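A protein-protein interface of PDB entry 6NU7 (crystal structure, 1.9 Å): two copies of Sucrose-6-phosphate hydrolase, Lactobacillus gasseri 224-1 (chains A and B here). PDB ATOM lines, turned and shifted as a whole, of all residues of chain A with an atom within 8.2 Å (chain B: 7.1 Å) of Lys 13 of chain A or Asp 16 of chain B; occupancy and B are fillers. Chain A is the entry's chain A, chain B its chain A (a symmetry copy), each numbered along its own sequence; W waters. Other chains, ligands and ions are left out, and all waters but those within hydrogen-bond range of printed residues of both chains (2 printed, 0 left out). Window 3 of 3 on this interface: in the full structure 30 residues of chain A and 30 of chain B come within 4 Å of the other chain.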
ATOM      1  N   ARG A  10       9.556  18.977   1.115  1.00  0.00           N
ATOM      2  CA  ARG A  10      10.479  17.945   1.558  1.00  0.00           C
ATOM      3  C   ARG A  10       9.788  16.577   1.515  1.00  0.00           C
ATOM      4  O   ARG A  10       8.608  16.435   1.874  1.00  0.00           O
ATOM      5  CB  ARG A  10      10.984  18.278   2.969  1.00  0.00           C
ATOM      6  CG  ARG A  10      12.213  17.523   3.416  1.00  0.00           C
ATOM      7  CD  ARG A  10      12.966  18.311   4.499  1.00  0.00           C
ATOM      8  NE  ARG A  10      12.240  18.243   5.765  1.00  0.00           N
ATOM      9  CZ  ARG A  10      12.696  17.619   6.849  1.00  0.00           C
ATOM     10  NH1 ARG A  10      13.880  17.014   6.809  1.00  0.00           N
ATOM     11  NH2 ARG A  10      11.980  17.604   7.975  1.00  0.00           N
ATOM     12  N   LYS A  11      10.501  15.577   1.005  1.00  0.00           N
ATOM     13  CA  LYS A  11       9.892  14.255   0.845  1.00  0.00           C
ATOM     14  C   LYS A  11       9.641  13.601   2.202  1.00  0.00           C
ATOM     15  O   LYS A  11      10.330  13.886   3.192  1.00  0.00           O
ATOM     16  CB  LYS A  11      10.785  13.353  -0.004  1.00  0.00           C
ATOM     17  CG  LYS A  11      11.128  13.954  -1.358  1.00  0.00           C
ATOM     18  CD  LYS A  11      11.882  12.958  -2.195  1.00  0.00           C
ATOM     19  CE  LYS A  11      10.933  11.926  -2.791  1.00  0.00           C
ATOM     20  NZ  LYS A  11       9.957  12.528  -3.746  1.00  0.00           N
ATOM     21  N   TYR A  12       8.639  12.710   2.245  1.00  0.00           N
ATOM     22  CA  TYR A  12       8.349  12.031   3.507  1.00  0.00           C
ATOM     23  C   TYR A  12       9.563  11.269   4.022  1.00  0.00           C
ATOM     24  O   TYR A  12       9.761  11.181   5.239  1.00  0.00           O
ATOM     25  CB  TYR A  12       7.174  11.062   3.362  1.00  0.00           C
ATOM     26  CG  TYR A  12       5.832  11.683   3.016  1.00  0.00           C
ATOM     27  CD1 TYR A  12       5.674  13.070   2.845  1.00  0.00           C
ATOM     28  CD2 TYR A  12       4.723  10.870   2.832  1.00  0.00           C
ATOM     29  CE1 TYR A  12       4.426  13.627   2.501  1.00  0.00           C
ATOM     30  CE2 TYR A  12       3.480  11.419   2.501  1.00  0.00           C
ATOM     31  CZ  TYR A  12       3.329  12.780   2.337  1.00  0.00           C
ATOM     32  OH  TYR A  12       2.061  13.253   2.007  1.00  0.00           O
ATOM     33  N   LYS A  13      10.379  10.707   3.120  1.00  0.00           N
ATOM     34  CA  LYS A  13      11.569   9.972   3.547  1.00  0.00           C
ATOM     35  C   LYS A  13      12.617  10.877   4.168  1.00  0.00           C
ATOM     36  O   LYS A  13      13.576  10.371   4.767  1.00  0.00           O
ATOM     37  CB  LYS A  13      12.204   9.232   2.372  1.00  0.00           C
ATOM     38  CG  LYS A  13      12.562  10.180   1.226  1.00  0.00           C
ATOM     39  CD  LYS A  13      13.888   9.816   0.536  1.00  0.00           C
ATOM     40  CE  LYS A  13      13.668   8.918  -0.666  1.00  0.00           C
ATOM     41  N   ASP A  14      12.488  12.191   4.007  1.00  0.00           N
ATOM     42  CA  ASP A  14      13.442  13.110   4.619  1.00  0.00           C
ATOM     43  C   ASP A  14      12.999  13.595   6.001  1.00  0.00           C
ATOM     44  O   ASP A  14      13.721  14.376   6.638  1.00  0.00           O
ATOM     45  CB  ASP A  14      13.692  14.292   3.671  1.00  0.00           C
ATOM     46  CG  ASP A  14      14.472  13.874   2.429  1.00  0.00           C
ATOM     47  OD1 ASP A  14      15.314  12.943   2.506  1.00  0.00           O
ATOM     48  OD2 ASP A  14      14.240  14.477   1.378  1.00  0.00           O
ATOM     49  N   TRP A  15      11.821  13.184   6.453  1.00  0.00           N
ATOM     50  CA  TRP A  15      11.430  13.294   7.848  1.00  0.00           C
ATOM     51  C   TRP A  15      11.850  12.023   8.586  1.00  0.00           C
ATOM     52  O   TRP A  15      11.890  10.933   8.007  1.00  0.00           O
ATOM     53  CB  TRP A  15       9.918  13.493   7.958  1.00  0.00           C
ATOM     54  CG  TRP A  15       9.465  14.836   7.511  1.00  0.00           C
ATOM     55  CD1 TRP A  15       9.264  15.269   6.217  1.00  0.00           C
ATOM     56  CD2 TRP A  15       9.160  15.942   8.357  1.00  0.00           C
ATOM     57  NE1 TRP A  15       8.821  16.584   6.226  1.00  0.00           N
ATOM     58  CE2 TRP A  15       8.770  17.019   7.524  1.00  0.00           C
ATOM     59  CE3 TRP A  15       9.181  16.128   9.743  1.00  0.00           C
ATOM     60  CZ2 TRP A  15       8.430  18.266   8.033  1.00  0.00           C
ATOM     61  CZ3 TRP A  15       8.800  17.357  10.248  1.00  0.00           C
ATOM     62  CH2 TRP A  15       8.438  18.417   9.389  1.00  0.00           C
ATOM     63  N   ASP A  16      12.161  12.159   9.859  1.00  0.00           N
ATOM     64  CA  ASP A  16      12.494  10.968  10.622  1.00  0.00           C
ATOM     65  C   ASP A  16      11.244  10.376  11.271  1.00  0.00           C
ATOM     66  O   ASP A  16      10.217  11.055  11.470  1.00  0.00           O
ATOM     67  CB  ASP A  16      13.541  11.278  11.685  1.00  0.00           C
ATOM     68  CG  ASP A  16      12.971  12.079  12.830  1.00  0.00           C
ATOM     69  OD1 ASP A  16      12.914  13.321  12.720  1.00  0.00           O
ATOM     70  OD2 ASP A  16      12.563  11.464  13.835  1.00  0.00           O
ATOM     71  N   ALA A  17      11.350   9.088  11.623  1.00  0.00           N
ATOM     72  CA  ALA A  17      10.189   8.357  12.131  1.00  0.00           C
ATOM     73  C   ALA A  17       9.838   8.759  13.555  1.00  0.00           C
ATOM     74  O   ALA A  17       8.660   8.703  13.942  1.00  0.00           O
ATOM     75  CB  ALA A  17      10.429   6.851  12.058  1.00  0.00           C
ATOM     76  N   GLN A  18      10.839   9.144  14.351  1.00  0.00           N
ATOM     77  CA  GLN A  18      10.548   9.615  15.703  1.00  0.00           C
ATOM     78  C   GLN A  18       9.659  10.849  15.662  1.00  0.00           C
ATOM     79  O   GLN A  18       8.696  10.957  16.433  1.00  0.00           O
ATOM     80  CB  GLN A  18      11.827   9.933  16.472  1.00  0.00           C
ATOM     81  CG  GLN A  18      11.556  10.526  17.857  1.00  0.00           C
ATOM     82  CD  GLN A  18      11.158   9.446  18.860  1.00  0.00           C
ATOM     83  OE1 GLN A  18      11.903   8.488  19.056  1.00  0.00           O
ATOM     84  NE2 GLN A  18       9.983   9.593  19.488  1.00  0.00           N
ATOM     85  N   THR A  19       9.968  11.793  14.764  1.00  0.00           N
ATOM     86  CA  THR A  19       9.123  12.981  14.640  1.00  0.00           C
ATOM     87  C   THR A  19       7.688  12.592  14.278  1.00  0.00           C
ATOM     88  O   THR A  19       6.728  13.094  14.879  1.00  0.00           O
ATOM     89  CB  THR A  19       9.726  13.945  13.609  1.00  0.00           C
ATOM     90  OG1 THR A  19      11.023  14.346  14.061  1.00  0.00           O
ATOM     91  CG2 THR A  19       8.824  15.208  13.376  1.00  0.00           C
ATOM     92  N   LEU A  20       7.518  11.671  13.327  1.00  0.00           N
ATOM     93  CA  LEU A  20       6.167  11.236  12.984  1.00  0.00           C
ATOM     94  C   LEU A  20       5.454  10.583  14.174  1.00  0.00           C
ATOM     95  O   LEU A  20       4.269  10.837  14.401  1.00  0.00           O
ATOM     96  CB  LEU A  20       6.201  10.275  11.798  1.00  0.00           C
ATOM     97  CG  LEU A  20       4.852   9.683  11.347  1.00  0.00           C
ATOM     98  CD1 LEU A  20       3.810  10.758  11.049  1.00  0.00           C
ATOM     99  CD2 LEU A  20       5.075   8.827  10.105  1.00  0.00           C
ATOM    100  N   PHE A  67       2.935  15.738   8.455  1.00  0.00           N
ATOM    101  CA  PHE A  67       4.028  16.246   9.276  1.00  0.00           C
ATOM    102  C   PHE A  67       3.790  17.625   9.856  1.00  0.00           C
ATOM    103  O   PHE A  67       4.695  18.173  10.485  1.00  0.00           O
ATOM    104  CB  PHE A  67       5.326  16.252   8.470  1.00  0.00           C
ATOM    105  CG  PHE A  67       5.727  14.892   8.018  1.00  0.00           C
ATOM    106  CD1 PHE A  67       6.292  13.990   8.911  1.00  0.00           C
ATOM    107  CD2 PHE A  67       5.494  14.485   6.711  1.00  0.00           C
ATOM    108  CE1 PHE A  67       6.650  12.720   8.488  1.00  0.00           C
ATOM    109  CE2 PHE A  67       5.837  13.224   6.287  1.00  0.00           C
ATOM    110  CZ  PHE A  67       6.410  12.336   7.166  1.00  0.00           C
ATOM    111  N   ARG B  10      18.801   0.358  16.778  1.00  0.00           N
ATOM    112  CA  ARG B  10      18.790   1.640  16.094  1.00  0.00           C
ATOM    113  C   ARG B  10      17.637   2.501  16.623  1.00  0.00           C
ATOM    114  O   ARG B  10      16.523   2.012  16.868  1.00  0.00           O
ATOM    115  CB  ARG B  10      18.679   1.416  14.580  1.00  0.00           C
ATOM    116  CG  ARG B  10      19.028   2.605  13.718  1.00  0.00           C
ATOM    117  CD  ARG B  10      19.472   2.146  12.320  1.00  0.00           C
ATOM    118  NE  ARG B  10      18.315   1.696  11.549  1.00  0.00           N
ATOM    119  CZ  ARG B  10      17.857   2.320  10.465  1.00  0.00           C
ATOM    120  NH1 ARG B  10      18.469   3.418  10.033  1.00  0.00           N
ATOM    121  NH2 ARG B  10      16.798   1.846   9.807  1.00  0.00           N
ATOM    122  N   TYR B  12      14.585   5.212  16.998  1.00  0.00           N
ATOM    123  CA  TYR B  12      13.462   5.503  16.109  1.00  0.00           C
ATOM    124  C   TYR B  12      13.766   6.682  15.194  1.00  0.00           C
ATOM    125  O   TYR B  12      13.312   6.699  14.044  1.00  0.00           O
ATOM    126  CB  TYR B  12      12.185   5.797  16.898  1.00  0.00           C
ATOM    127  CG  TYR B  12      11.641   4.657  17.741  1.00  0.00           C
ATOM    128  CD1 TYR B  12      12.268   3.398  17.789  1.00  0.00           C
ATOM    129  CD2 TYR B  12      10.506   4.852  18.515  1.00  0.00           C
ATOM    130  CE1 TYR B  12      11.761   2.359  18.594  1.00  0.00           C
ATOM    131  CE2 TYR B  12       9.994   3.820  19.308  1.00  0.00           C
ATOM    132  CZ  TYR B  12      10.611   2.588  19.350  1.00  0.00           C
ATOM    133  OH  TYR B  12      10.043   1.609  20.163  1.00  0.00           O
ATOM    134  N   LYS B  13      14.519   7.675  15.683  1.00  0.00           N
ATOM    135  CA  LYS B  13      14.859   8.831  14.854  1.00  0.00           C
ATOM    136  C   LYS B  13      15.791   8.471  13.712  1.00  0.00           C
ATOM    137  O   LYS B  13      15.988   9.295  12.808  1.00  0.00           O
ATOM    138  CB  LYS B  13      15.517   9.928  15.688  1.00  0.00           C
ATOM    139  CG  LYS B  13      16.767   9.421  16.411  1.00  0.00           C
ATOM    140  CD  LYS B  13      17.899  10.462  16.454  1.00  0.00           C
ATOM    141  CE  LYS B  13      17.856  11.288  17.726  1.00  0.00           C
ATOM    142  N   ASP B  14      16.400   7.289  13.746  1.00  0.00           N
ATOM    143  CA  ASP B  14      17.272   6.873  12.654  1.00  0.00           C
ATOM    144  C   ASP B  14      16.539   6.064  11.581  1.00  0.00           C
ATOM    145  O   ASP B  14      17.161   5.653  10.590  1.00  0.00           O
ATOM    146  CB  ASP B  14      18.463   6.087  13.222  1.00  0.00           C
ATOM    147  CG  ASP B  14      19.416   6.981  14.008  1.00  0.00           C
ATOM    148  OD1 ASP B  14      19.562   8.184  13.671  1.00  0.00           O
ATOM    149  OD2 ASP B  14      20.016   6.480  14.962  1.00  0.00           O
ATOM    150  N   TRP B  15      15.254   5.798  11.777  1.00  0.00           N
ATOM    151  CA  TRP B  15      14.374   5.337  10.716  1.00  0.00           C
ATOM    152  C   TRP B  15      13.737   6.549  10.036  1.00  0.00           C
ATOM    153  O   TRP B  15      13.510   7.588  10.664  1.00  0.00           O
ATOM    154  CB  TRP B  15      13.290   4.425  11.290  1.00  0.00           C
ATOM    155  CG  TRP B  15      13.803   3.098  11.721  1.00  0.00           C
ATOM    156  CD1 TRP B  15      14.456   2.789  12.896  1.00  0.00           C
ATOM    157  CD2 TRP B  15      13.717   1.884  10.978  1.00  0.00           C
ATOM    158  NE1 TRP B  15      14.753   1.434  12.926  1.00  0.00           N
ATOM    159  CE2 TRP B  15      14.327   0.868  11.753  1.00  0.00           C
ATOM    160  CE3 TRP B  15      13.186   1.557   9.726  1.00  0.00           C
ATOM    161  CZ2 TRP B  15      14.438  -0.442  11.304  1.00  0.00           C
ATOM    162  CZ3 TRP B  15      13.260   0.245   9.302  1.00  0.00           C
ATOM    163  CH2 TRP B  15      13.893  -0.741  10.090  1.00  0.00           C
ATOM    164  N   ASP B  16      13.450   6.419   8.757  1.00  0.00           N
ATOM    165  CA  ASP B  16      12.776   7.516   8.084  1.00  0.00           C
ATOM    166  C   ASP B  16      11.259   7.347   8.162  1.00  0.00           C
ATOM    167  O   ASP B  16      10.727   6.240   8.374  1.00  0.00           O
ATOM    168  CB  ASP B  16      13.218   7.616   6.628  1.00  0.00           C
ATOM    169  CG  ASP B  16      12.650   6.502   5.782  1.00  0.00           C
ATOM    170  OD1 ASP B  16      13.256   5.411   5.748  1.00  0.00           O
ATOM    171  OD2 ASP B  16      11.588   6.713   5.164  1.00  0.00           O
ATOM    172  N   ALA B  17      10.557   8.471   7.967  1.00  0.00           N
ATOM    173  CA  ALA B  17       9.105   8.484   8.147  1.00  0.00           C
ATOM    174  C   ALA B  17       8.383   7.786   7.006  1.00  0.00           C
ATOM    175  O   ALA B  17       7.297   7.220   7.214  1.00  0.00           O
ATOM    176  CB  ALA B  17       8.595   9.915   8.291  1.00  0.00           C
ATOM    177  N   GLN B  18       8.948   7.832   5.797  1.00  0.00           N
ATOM    178  CA  GLN B  18       8.336   7.113   4.683  1.00  0.00           C
ATOM    179  C   GLN B  18       8.284   5.620   4.972  1.00  0.00           C
ATOM    180  O   GLN B  18       7.263   4.966   4.723  1.00  0.00           O
ATOM    181  CB  GLN B  18       9.091   7.355   3.379  1.00  0.00           C
ATOM    182  CG  GLN B  18       8.536   6.534   2.211  1.00  0.00           C
ATOM    183  CD  GLN B  18       7.259   7.153   1.649  1.00  0.00           C
ATOM    184  OE1 GLN B  18       7.265   8.319   1.255  1.00  0.00           O
ATOM    185  NE2 GLN B  18       6.164   6.381   1.619  1.00  0.00           N
ATOM    186  N   THR B  19       9.382   5.063   5.499  1.00  0.00           N
ATOM    187  CA  THR B  19       9.378   3.641   5.846  1.00  0.00           C
ATOM    188  C   THR B  19       8.286   3.336   6.874  1.00  0.00           C
ATOM    189  O   THR B  19       7.534   2.362   6.723  1.00  0.00           O
ATOM    190  CB  THR B  19      10.766   3.225   6.354  1.00  0.00           C
ATOM    191  OG1 THR B  19      11.719   3.443   5.309  1.00  0.00           O
ATOM    192  CG2 THR B  19      10.806   1.725   6.814  1.00  0.00           C
ATOM    193  N   LEU B  20       8.154   4.173   7.904  1.00  0.00           N
ATOM    194  CA  LEU B  20       7.093   3.944   8.881  1.00  0.00           C
ATOM    195  C   LEU B  20       5.700   4.018   8.247  1.00  0.00           C
ATOM    196  O   LEU B  20       4.833   3.199   8.559  1.00  0.00           O
ATOM    197  CB  LEU B  20       7.202   4.945  10.030  1.00  0.00           C
ATOM    198  CG  LEU B  20       6.118   4.867  11.122  1.00  0.00           C
ATOM    199  CD1 LEU B  20       5.993   3.471  11.726  1.00  0.00           C
ATOM    200  CD2 LEU B  20       6.443   5.875  12.219  1.00  0.00           C
ATOM    201  N   LEU B  21       5.448   5.014   7.386  1.00  0.00           N
ATOM    202  CA  LEU B  21       4.144   5.066   6.724  1.00  0.00           C
ATOM    203  C   LEU B  21       3.913   3.813   5.872  1.00  0.00           C
ATOM    204  O   LEU B  21       2.817   3.231   5.891  1.00  0.00           O
ATOM    205  CB  LEU B  21       4.027   6.348   5.885  1.00  0.00           C
ATOM    206  CG  LEU B  21       3.897   7.583   6.802  1.00  0.00           C
ATOM    207  CD1 LEU B  21       4.306   8.852   6.065  1.00  0.00           C
ATOM    208  CD2 LEU B  21       2.485   7.714   7.417  1.00  0.00           C
ATOM    209  N   ASP B  22       4.944   3.361   5.144  1.00  0.00           N
ATOM    210  CA  ASP B  22       4.804   2.139   4.352  1.00  0.00           C
ATOM    211  C   ASP B  22       4.431   0.968   5.250  1.00  0.00           C
ATOM    212  O   ASP B  22       3.577   0.138   4.902  1.00  0.00           O
ATOM    213  CB  ASP B  22       6.109   1.804   3.623  1.00  0.00           C
ATOM    214  CG  ASP B  22       6.492   2.824   2.571  1.00  0.00           C
ATOM    215  OD1 ASP B  22       5.640   3.611   2.116  1.00  0.00           O
ATOM    216  OD2 ASP B  22       7.677   2.816   2.195  1.00  0.00           O
ATOM    217  N   LEU B  23       5.075   0.886   6.416  1.00  0.00           N
ATOM    218  CA  LEU B  23       4.840  -0.232   7.325  1.00  0.00           C
ATOM    219  C   LEU B  23       3.429  -0.200   7.891  1.00  0.00           C
ATOM    220  O   LEU B  23       2.854  -1.264   8.184  1.00  0.00           O
ATOM    221  CB  LEU B  23       5.869  -0.209   8.464  1.00  0.00           C
ATOM    222  CG  LEU B  23       7.310  -0.629   8.065  1.00  0.00           C
ATOM    223  CD1 LEU B  23       8.303  -0.277   9.176  1.00  0.00           C
ATOM    224  CD2 LEU B  23       7.345  -2.158   7.760  1.00  0.00           C
ATOM    225  N   PHE B  67       8.925  -0.942  13.779  1.00  0.00           N
ATOM    226  CA  PHE B  67       9.608  -0.962  12.491  1.00  0.00           C
ATOM    227  C   PHE B  67       9.827  -2.347  11.916  1.00  0.00           C
ATOM    228  O   PHE B  67      10.477  -2.466  10.878  1.00  0.00           O
ATOM    229  CB  PHE B  67      10.951  -0.241  12.602  1.00  0.00           C
ATOM    230  CG  PHE B  67      10.806   1.189  12.987  1.00  0.00           C
ATOM    231  CD1 PHE B  67      10.383   2.130  12.056  1.00  0.00           C
ATOM    232  CD2 PHE B  67      11.036   1.595  14.295  1.00  0.00           C
ATOM    233  CE1 PHE B  67      10.235   3.457  12.424  1.00  0.00           C
ATOM    234  CE2 PHE B  67      10.881   2.908  14.669  1.00  0.00           C
ATOM    235  CZ  PHE B  67      10.478   3.842  13.745  1.00  0.00           C
HETATM  236  O   HOH W   1       9.296   9.934   0.520  1.00  0.00           O
HETATM  237  O   HOH W   2      14.534   8.155  18.564  1.00  0.00           O
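Water W2 lies within hydrogen-bond range of the side-chain amide oxygen (OE1) of Gln 18 of chain A (2.7 Å), the backbone NH (N) of Lys 13 of chain B (2.9 Å) and the backbone NH (N) of Tyr 12 of chain B (3.3 Å).
Water W1 lies within hydrogen-bond range of OE1 of Gln 18 of chain B (2.7 Å), N of Lys 13 of chain A (2.9 Å) and N of Tyr 12 of chain A (3.3 Å).
Lys 13 of chain A touches just these residues of chain B: Asp 16 (3.3 Å) and Gln 18 (3.6 Å).
Asp 16 of chain B touches just these residues of chain A: Lys 13 (3.3 Å), Trp 15 (3.5 Å) and Ala 17 (3.7 Å).
Printed residues of chain A within 4 Å of Gln 18 of chain B: Tyr 12 (3.5 Å) and Lys 13 (3.6 Å).
Printed residues of chain B within 4 Å of Ala 17 of chain A: Tyr 12, Trp 15, Asp 16, Ala 17, Leu 20 and Phe 67.
Asp 22 of chain B touches none of the printed residues of chain A.
Thr 19 of chain B touches none of the printed residues of chain A.
The nearest residue of chain B that does not touch Lys 13 of chain A is Ala 17 of chain B (4.8 Å).
The nearest residue of chain A that does not touch Asp 16 of chain B is Asp 16 of chain A (4.3 Å).
The backbone NH of Gln 18 of chain B is in hydrogen-bond range of the backbone carbonyl oxygen of Tyr 12 of chain A (3.5 Å).
O of Trp 15 of chain A lies within hydrogen-bond range of N of Ala 17 of chain B (2.8 Å).
N of Ala 17 of chain A lies within hydrogen-bond range of O of Trp 15 of chain B (2.8 Å).
The backbone carbonyl oxygen (O) of Tyr 12 of chain B sits at hydrogen-bond distance from the backbone NH (N) of Gln 18 of chain A.
O of Tyr 12 of chain A touches CB of Ala 17 of chain B, 3.5 Å away.
CB of Asp 16 of chain B touches O of Lys 13 of chain A, 3.3 Å away.
Asp 16 of chain A touches Lys 13 of chain B.
Asp 16 of chain A touches Ala 17 of chain B.
CB of Ala 17 of chain A touches O of Tyr 12 of chain B, at 3.5 Å.
Ala 17 of chain A touches Asp 16 of chain B.
Ala 17 of chain B touches Ala 17 of chain A (N to N, 3.8 Å).
Ala 17 of chain A touches Leu 20 of chain B (O to CD2, 3.99 Å).
Phe 67 of chain B touches Ala 17 of chain A (CE1 to CB, 3.4 Å).
Gln 18 of chain A touches Lys 13 of chain B.
Printed residues of chain B that touch a printed residue of chain A: Tyr 12, Lys 13, Trp 15, Asp 16, Ala 17, Gln 18, Leu 20, Leu 21 and Phe 67.
Of the 12 printed residues of chain A, 8 touch a printed residue of chain B.
Printed residues of chain A that touch a printed residue of chain B: Tyr 12, Lys 13, Trp 15, Asp 16, Ala 17, Gln 18, Leu 20 and Phe 67.
Among the printed residues, 22 pairs touch across the chains.
Among the printed residues, no Asp or Glu carboxylate lies within 4 Å of a Lys or Arg side-chain nitrogen of the other chain.
N of Gln 18 of chain A sits at hydrogen-bond distance from OD2 of Asp 16 of chain A.
OG1 of Thr 19 of chain A is in hydrogen-bond range of OD1 of Asp 16 of chain A, 2.5 Å away.
N of Gln 18 of chain B sits at hydrogen-bond distance from OD2 of Asp 16 of chain B, at 2.9 Å.
The side-chain carboxylate of Asp 16 of chain B lies within hydrogen-bond range of the side-chain hydroxyl of Thr 19 of chain B, at 2.5 Å.
OD1 of Asp 22 of chain B sits at hydrogen-bond distance from NE2 of Gln 18 of chain B.
Lys 13 of chain A touches Asp 16 of chain B, and with the chains exchanged Asp 16 of chain A touches Lys 13 of chain B.
Ala 17 of chain A touches Leu 20 of chain B, and with the chains exchanged Leu 20 of chain A touches Ala 17 of chain B.
Ala 17 of chain A touches Phe 67 of chain B, and with the chains exchanged Phe 67 of chain A touches Ala 17 of chain B.
Leu 20 of chain A touches its own counterpart, Leu 20 of chain B.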
